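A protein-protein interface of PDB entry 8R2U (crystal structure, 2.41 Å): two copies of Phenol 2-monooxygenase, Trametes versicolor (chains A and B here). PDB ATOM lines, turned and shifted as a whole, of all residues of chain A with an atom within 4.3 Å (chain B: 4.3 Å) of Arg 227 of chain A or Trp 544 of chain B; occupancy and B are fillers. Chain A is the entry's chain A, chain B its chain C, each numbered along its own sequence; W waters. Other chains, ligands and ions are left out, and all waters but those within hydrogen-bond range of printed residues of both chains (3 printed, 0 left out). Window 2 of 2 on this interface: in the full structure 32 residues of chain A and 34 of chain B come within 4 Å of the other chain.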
ATOM      1  N   ASN A  77       3.356  18.885  12.063  1.00  0.00           N
ATOM      2  CA  ASN A  77       4.138  18.439  10.926  1.00  0.00           C
ATOM      3  C   ASN A  77       3.711  17.021  10.524  1.00  0.00           C
ATOM      4  O   ASN A  77       3.436  16.184  11.393  1.00  0.00           O
ATOM      5  CB  ASN A  77       5.629  18.487  11.283  1.00  0.00           C
ATOM      6  CG  ASN A  77       6.489  17.879  10.191  1.00  0.00           C
ATOM      7  OD1 ASN A  77       6.752  18.516   9.169  1.00  0.00           O
ATOM      8  ND2 ASN A  77       6.940  16.649  10.400  1.00  0.00           N
ATOM      9  N   ASP A 225      16.912  14.444   3.124  1.00  0.00           N
ATOM     10  CA  ASP A 225      15.770  13.763   3.702  1.00  0.00           C
ATOM     11  C   ASP A 225      15.537  14.289   5.118  1.00  0.00           C
ATOM     12  O   ASP A 225      14.990  13.590   5.979  1.00  0.00           O
ATOM     13  CB  ASP A 225      15.953  12.246   3.609  1.00  0.00           C
ATOM     14  CG  ASP A 225      15.779  11.698   2.204  1.00  0.00           C
ATOM     15  OD1 ASP A 225      14.642  11.807   1.667  1.00  0.00           O
ATOM     16  OD2 ASP A 225      16.764  11.138   1.682  1.00  0.00           O
ATOM     17  N   VAL A 226      15.851  15.571   5.311  1.00  0.00           N
ATOM     18  CA  VAL A 226      15.722  16.215   6.604  1.00  0.00           C
ATOM     19  C   VAL A 226      14.257  16.305   7.038  1.00  0.00           C
ATOM     20  O   VAL A 226      14.004  16.502   8.212  1.00  0.00           O
ATOM     21  CB  VAL A 226      16.370  17.600   6.536  1.00  0.00           C
ATOM     22  CG1 VAL A 226      15.496  18.561   5.730  1.00  0.00           C
ATOM     23  CG2 VAL A 226      16.683  18.120   7.939  1.00  0.00           C
ATOM     24  N   ARG A 227      13.306  16.163   6.105  1.00  0.00           N
ATOM     25  CA  ARG A 227      11.886  16.203   6.426  1.00  0.00           C
ATOM     26  C   ARG A 227      11.261  14.795   6.392  1.00  0.00           C
ATOM     27  O   ARG A 227      10.036  14.632   6.412  1.00  0.00           O
ATOM     28  CB  ARG A 227      11.125  17.110   5.451  1.00  0.00           C
ATOM     29  CG  ARG A 227      11.659  18.524   5.310  1.00  0.00           C
ATOM     30  CD  ARG A 227      11.912  19.191   6.633  1.00  0.00           C
ATOM     31  NE  ARG A 227      10.707  19.174   7.420  1.00  0.00           N
ATOM     32  CZ  ARG A 227      10.647  19.482   8.724  1.00  0.00           C
ATOM     33  NH1 ARG A 227      11.718  19.919   9.387  1.00  0.00           N
ATOM     34  NH2 ARG A 227       9.489  19.378   9.368  1.00  0.00           N
ATOM     35  N   CYS A 228      12.124  13.773   6.388  1.00  0.00           N
ATOM     36  CA  CYS A 228      11.711  12.392   6.560  1.00  0.00           C
ATOM     37  C   CYS A 228      12.099  11.871   7.944  1.00  0.00           C
ATOM     38  O   CYS A 228      13.117  12.284   8.504  1.00  0.00           O
ATOM     39  CB  CYS A 228      12.374  11.482   5.535  1.00  0.00           C
ATOM     40  SG  CYS A 228      11.923  11.828   3.821  1.00  0.00           S
ATOM     41  N   PRO A 243      11.353  14.749  12.037  1.00  0.00           N
ATOM     42  CA  PRO A 243      10.986  16.115  11.665  1.00  0.00           C
ATOM     43  C   PRO A 243       9.819  16.618  12.511  1.00  0.00           C
ATOM     44  O   PRO A 243       8.947  15.827  12.882  1.00  0.00           O
ATOM     45  CB  PRO A 243      10.618  16.014  10.168  1.00  0.00           C
ATOM     46  CG  PRO A 243      10.362  14.535   9.929  1.00  0.00           C
ATOM     47  CD  PRO A 243      11.231  13.801  10.916  1.00  0.00           C
ATOM     48  N   ARG A 244       9.839  17.924  12.819  1.00  0.00           N
ATOM     49  CA  ARG A 244       8.912  18.559  13.747  1.00  0.00           C
ATOM     50  C   ARG A 244       8.255  19.776  13.101  1.00  0.00           C
ATOM     51  O   ARG A 244       8.375  19.999  11.905  1.00  0.00           O
ATOM     52  CB  ARG A 244       9.690  18.957  14.996  1.00  0.00           C
ATOM     53  CG  ARG A 244      10.041  17.765  15.880  1.00  0.00           C
ATOM     54  CD  ARG A 244       8.928  17.388  16.831  1.00  0.00           C
ATOM     55  NE  ARG A 244       8.660  18.515  17.711  1.00  0.00           N
ATOM     56  CZ  ARG A 244       9.472  18.962  18.642  1.00  0.00           C
ATOM     57  NH1 ARG A 244      10.311  18.153  19.246  1.00  0.00           N
ATOM     58  NH2 ARG A 244       9.359  20.207  19.042  1.00  0.00           N
ATOM     59  N   GLY A 246       7.247  23.253  11.592  1.00  0.00           N
ATOM     60  CA  GLY A 246       8.041  24.231  10.864  1.00  0.00           C
ATOM     61  C   GLY A 246       9.285  23.593  10.252  1.00  0.00           C
ATOM     62  O   GLY A 246       9.170  22.598   9.551  1.00  0.00           O
ATOM     63  N   ASP A 247      10.461  24.165  10.544  1.00  0.00           N
ATOM     64  CA  ASP A 247      11.736  23.682  10.026  1.00  0.00           C
ATOM     65  C   ASP A 247      12.470  22.800  11.046  1.00  0.00           C
ATOM     66  O   ASP A 247      13.522  22.233  10.712  1.00  0.00           O
ATOM     67  CB  ASP A 247      12.659  24.844   9.664  1.00  0.00           C
ATOM     68  CG  ASP A 247      12.193  25.681   8.490  1.00  0.00           C
ATOM     69  OD1 ASP A 247      11.288  25.212   7.765  1.00  0.00           O
ATOM     70  OD2 ASP A 247      12.737  26.788   8.340  1.00  0.00           O
ATOM     71  N   LEU A 248      11.896  22.651  12.264  1.00  0.00           N
ATOM     72  CA  LEU A 248      12.581  21.994  13.356  1.00  0.00           C
ATOM     73  C   LEU A 248      12.650  20.499  13.076  1.00  0.00           C
ATOM     74  O   LEU A 248      11.788  19.952  12.384  1.00  0.00           O
ATOM     75  CB  LEU A 248      11.842  22.221  14.670  1.00  0.00           C
ATOM     76  CG  LEU A 248      11.731  23.659  15.184  1.00  0.00           C
ATOM     77  CD1 LEU A 248      10.928  23.682  16.496  1.00  0.00           C
ATOM     78  CD2 LEU A 248      13.099  24.337  15.376  1.00  0.00           C
ATOM     79  N   ILE A 249      13.715  19.881  13.606  1.00  0.00           N
ATOM     80  CA  ILE A 249      13.802  18.447  13.723  1.00  0.00           C
ATOM     81  C   ILE A 249      14.193  18.090  15.154  1.00  0.00           C
ATOM     82  O   ILE A 249      14.782  18.893  15.877  1.00  0.00           O
ATOM     83  CB  ILE A 249      14.812  17.902  12.716  1.00  0.00           C
ATOM     84  CG1 ILE A 249      16.258  18.190  13.136  1.00  0.00           C
ATOM     85  CG2 ILE A 249      14.494  18.452  11.339  1.00  0.00           C
ATOM     86  CD1 ILE A 249      17.325  17.804  12.092  1.00  0.00           C
ATOM     87  N   ARG B 455       4.917  17.549  -2.338  1.00  0.00           N
ATOM     88  CA  ARG B 455       6.211  18.117  -2.014  1.00  0.00           C
ATOM     89  C   ARG B 455       7.312  17.067  -2.117  1.00  0.00           C
ATOM     90  O   ARG B 455       7.137  15.968  -1.632  1.00  0.00           O
ATOM     91  CB  ARG B 455       6.160  18.653  -0.588  1.00  0.00           C
ATOM     92  CG  ARG B 455       5.650  20.077  -0.528  1.00  0.00           C
ATOM     93  CD  ARG B 455       4.818  20.390   0.671  1.00  0.00           C
ATOM     94  NE  ARG B 455       5.427  20.226   1.971  1.00  0.00           N
ATOM     95  CZ  ARG B 455       5.045  20.896   3.046  1.00  0.00           C
ATOM     96  NH1 ARG B 455       4.482  22.078   2.933  1.00  0.00           N
ATOM     97  NH2 ARG B 455       5.308  20.413   4.234  1.00  0.00           N
ATOM     98  N   ALA B 457      10.164  17.165  -0.571  1.00  0.00           N
ATOM     99  CA  ALA B 457      10.923  17.108   0.669  1.00  0.00           C
ATOM    100  C   ALA B 457      10.348  16.070   1.615  1.00  0.00           C
ATOM    101  O   ALA B 457      11.106  15.392   2.309  1.00  0.00           O
ATOM    102  CB  ALA B 457      10.889  18.456   1.320  1.00  0.00           C
ATOM    103  N   ASP B 458       9.012  15.968   1.644  1.00  0.00           N
ATOM    104  CA  ASP B 458       8.339  15.203   2.686  1.00  0.00           C
ATOM    105  C   ASP B 458       7.163  14.392   2.148  1.00  0.00           C
ATOM    106  O   ASP B 458       6.546  13.683   2.924  1.00  0.00           O
ATOM    107  CB  ASP B 458       7.895  16.093   3.854  1.00  0.00           C
ATOM    108  CG  ASP B 458       6.838  17.140   3.560  1.00  0.00           C
ATOM    109  OD1 ASP B 458       6.420  17.283   2.377  1.00  0.00           O
ATOM    110  OD2 ASP B 458       6.418  17.813   4.539  1.00  0.00           O
ATOM    111  N   TYR B 533      14.501  17.365  -2.960  1.00  0.00           N
ATOM    112  CA  TYR B 533      14.192  18.792  -3.013  1.00  0.00           C
ATOM    113  C   TYR B 533      15.472  19.569  -3.322  1.00  0.00           C
ATOM    114  O   TYR B 533      15.395  20.589  -4.008  1.00  0.00           O
ATOM    115  CB  TYR B 533      13.476  19.286  -1.753  1.00  0.00           C
ATOM    116  CG  TYR B 533      14.378  19.793  -0.665  1.00  0.00           C
ATOM    117  CD1 TYR B 533      14.892  21.079  -0.694  1.00  0.00           C
ATOM    118  CD2 TYR B 533      14.714  18.992   0.416  1.00  0.00           C
ATOM    119  CE1 TYR B 533      15.716  21.565   0.316  1.00  0.00           C
ATOM    120  CE2 TYR B 533      15.547  19.454   1.426  1.00  0.00           C
ATOM    121  CZ  TYR B 533      16.050  20.743   1.376  1.00  0.00           C
ATOM    122  OH  TYR B 533      16.898  21.177   2.338  1.00  0.00           O
ATOM    123  N   HIS B 543      12.570  27.961   0.051  1.00  0.00           N
ATOM    124  CA  HIS B 543      12.315  27.143   1.225  1.00  0.00           C
ATOM    125  C   HIS B 543      12.106  25.727   0.704  1.00  0.00           C
ATOM    126  O   HIS B 543      11.707  25.557  -0.434  1.00  0.00           O
ATOM    127  CB  HIS B 543      11.101  27.651   1.993  1.00  0.00           C
ATOM    128  CG  HIS B 543      10.786  26.895   3.245  1.00  0.00           C
ATOM    129  ND1 HIS B 543       9.789  25.942   3.322  1.00  0.00           N
ATOM    130  CD2 HIS B 543      11.359  26.945   4.451  1.00  0.00           C
ATOM    131  CE1 HIS B 543       9.762  25.449   4.549  1.00  0.00           C
ATOM    132  NE2 HIS B 543      10.718  26.031   5.246  1.00  0.00           N
ATOM    133  N   TRP B 544      12.372  24.710   1.527  1.00  0.00           N
ATOM    134  CA  TRP B 544      12.288  23.342   1.048  1.00  0.00           C
ATOM    135  C   TRP B 544      10.885  23.006   0.555  1.00  0.00           C
ATOM    136  O   TRP B 544      10.716  22.071  -0.213  1.00  0.00           O
ATOM    137  CB  TRP B 544      12.757  22.348   2.130  1.00  0.00           C
ATOM    138  CG  TRP B 544      12.092  22.472   3.473  1.00  0.00           C
ATOM    139  CD1 TRP B 544      12.620  23.043   4.595  1.00  0.00           C
ATOM    140  CD2 TRP B 544      10.798  21.960   3.841  1.00  0.00           C
ATOM    141  NE1 TRP B 544      11.736  22.951   5.626  1.00  0.00           N
ATOM    142  CE2 TRP B 544      10.608  22.288   5.203  1.00  0.00           C
ATOM    143  CE3 TRP B 544       9.789  21.271   3.167  1.00  0.00           C
ATOM    144  CZ2 TRP B 544       9.445  21.940   5.903  1.00  0.00           C
ATOM    145  CZ3 TRP B 544       8.661  20.914   3.862  1.00  0.00           C
ATOM    146  CH2 TRP B 544       8.486  21.246   5.210  1.00  0.00           C
ATOM    147  N   SER B 545       9.876  23.752   1.006  1.00  0.00           N
ATOM    148  CA  SER B 545       8.499  23.435   0.655  1.00  0.00           C
ATOM    149  C   SER B 545       8.111  23.952  -0.726  1.00  0.00           C
ATOM    150  O   SER B 545       7.008  23.706  -1.203  1.00  0.00           O
ATOM    151  CB  SER B 545       7.588  23.988   1.681  1.00  0.00           C
ATOM    152  OG  SER B 545       7.685  25.388   1.704  1.00  0.00           O
ATOM    153  N   LYS B 546       8.996  24.702  -1.370  1.00  0.00           N
ATOM    154  CA  LYS B 546       8.637  25.288  -2.648  1.00  0.00           C
ATOM    155  C   LYS B 546       8.797  24.266  -3.769  1.00  0.00           C
ATOM    156  O   LYS B 546       8.427  24.566  -4.911  1.00  0.00           O
ATOM    157  CB  LYS B 546       9.487  26.522  -2.931  1.00  0.00           C
ATOM    158  CG  LYS B 546       9.461  27.578  -1.832  1.00  0.00           C
ATOM    159  CD  LYS B 546       8.059  28.160  -1.645  1.00  0.00           C
ATOM    160  CE  LYS B 546       7.966  29.270  -0.629  1.00  0.00           C
ATOM    161  NZ  LYS B 546       6.545  29.544  -0.377  1.00  0.00           N
ATOM    162  N   VAL B 547       9.345  23.076  -3.461  1.00  0.00           N
ATOM    163  CA  VAL B 547       9.616  22.108  -4.503  1.00  0.00           C
ATOM    164  C   VAL B 547       8.456  21.145  -4.572  1.00  0.00           C
ATOM    165  O   VAL B 547       8.401  20.237  -3.762  1.00  0.00           O
ATOM    166  CB  VAL B 547      10.919  21.335  -4.266  1.00  0.00           C
ATOM    167  CG1 VAL B 547      11.117  20.259  -5.328  1.00  0.00           C
ATOM    168  CG2 VAL B 547      12.120  22.266  -4.207  1.00  0.00           C
HETATM  169  O   HOH W   1      13.442  16.313   3.260  1.00  0.00           O
HETATM  170  O   HOH W   2       7.874  13.337   5.786  1.00  0.00           O
HETATM  171  O   HOH W   3       8.299  17.966   6.839  1.00  0.00           O
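Among the printed residues, merely in contact across the chains: Arg 227 of chain A with Ala 457 of chain B (3.6 Å), Arg 227 of chain A with Asp 458 of chain B (3.6 Å), Arg 227 of chain A with Trp 544 of chain B (3.4 Å), Cys 228 of chain A with Ala 457 of chain B (3.96 Å) and Gly 246 of chain A with Trp 544 of chain B (3.7 Å).
No position is printed for both chains. Of the 7 pairs that touch across the chains among the printed residues, none has its exchanged pair printed and touching as well.
The side-chain amide oxygen (OD1) of Asn 77 of chain A is in hydrogen-bond range of the guanidinium group (NH2) of Arg 227 of chain A (2.9 Å). The backbone carbonyl oxygen (O) of Arg 244 of chain A sits at hydrogen-bond distance from the guanidinium group (NH2) of Arg 227 of chain A. NH1 of Arg 227 of chain A lies within hydrogen-bond range of O of Asp 247 of chain A (3.2 Å). The guanidinium group of Arg 227 of chain A lies within hydrogen-bond range of the backbone carbonyl oxygen of Leu 248 of chain A, at 3.0 Å. The guanidinium group of Arg 455 of chain B lies within salt-bridge range of the side-chain carboxylate of Asp 458 of chain B, 2.8 Å away. A ring nitrogen (ND1) of His 543 of chain B sits at hydrogen-bond distance from the side-chain hydroxyl (OG) of Ser 545 of chain B (2.7 Å).
Arg 227 of chain A touches just these residues of chain B: Ala 457 (3.6 Å), Asp 458 (3.6 Å) and Trp 544 (3.4 Å). Printed residues of chain B within 4 Å of Cys 228 of chain A: Ala 457. Arg 244 of chain A touches none of the printed residues of chain B. Of the printed residues of chain A, His 543 of chain B touches Asp 247 (2.7 Å). Trp 544 of chain B touches three residues of chain A. Lys 546 of chain B touches none of the printed residues of chain A. The nearest printed residue of chain B that does not touch Arg 227 of chain A is Tyr 533 of chain B (5.6 Å). The nearest printed residue of chain A that does not touch Asp 458 of chain B is Asn 77 of chain A (4.7 Å).
Water W2 lies within hydrogen-bond range of O of Arg 227 of chain A and O of Asp 458 of chain B. Water W1 lies within hydrogen-bond range of O of Ala 457 of chain B (2.7 Å), N of Arg 227 of chain A (2.9 Å) and N of Val 226 of chain A (3.2 Å). Water W3 lies within hydrogen-bond range of NE of Arg 227 of chain A, OD1 of Asn 77 of chain A and OD2 of Asp 458 of chain B.
A ring nitrogen (NE2) of His 543 of chain B is in hydrogen-bond range of the side-chain carboxylate (OD1) of Asp 247 of chain A (2.7 Å). The indole nitrogen (NE1) of Trp 544 of chain B is in hydrogen-bond range of the side-chain carboxylate (OD1) of Asp 247 of chain A (3.1 Å).
Of the 11 printed residues of chain A, 4 touch a printed residue of chain B. Printed residues of chain A that touch a printed residue of chain B: Arg 227, Cys 228, Gly 246 and Asp 247. Of the 9 printed residues of chain B, 4 touch a printed residue of chain A. Printed residues of chain B that touch a printed residue of chain A: Ala 457, Asp 458, His 543 and Trp 544. Among the printed residues, 7 pairs touch across the chains. Among the printed residues, no Asp or Glu carboxylate lies within 4 Å of a Lys or Arg side-chain nitrogen of the other chain.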
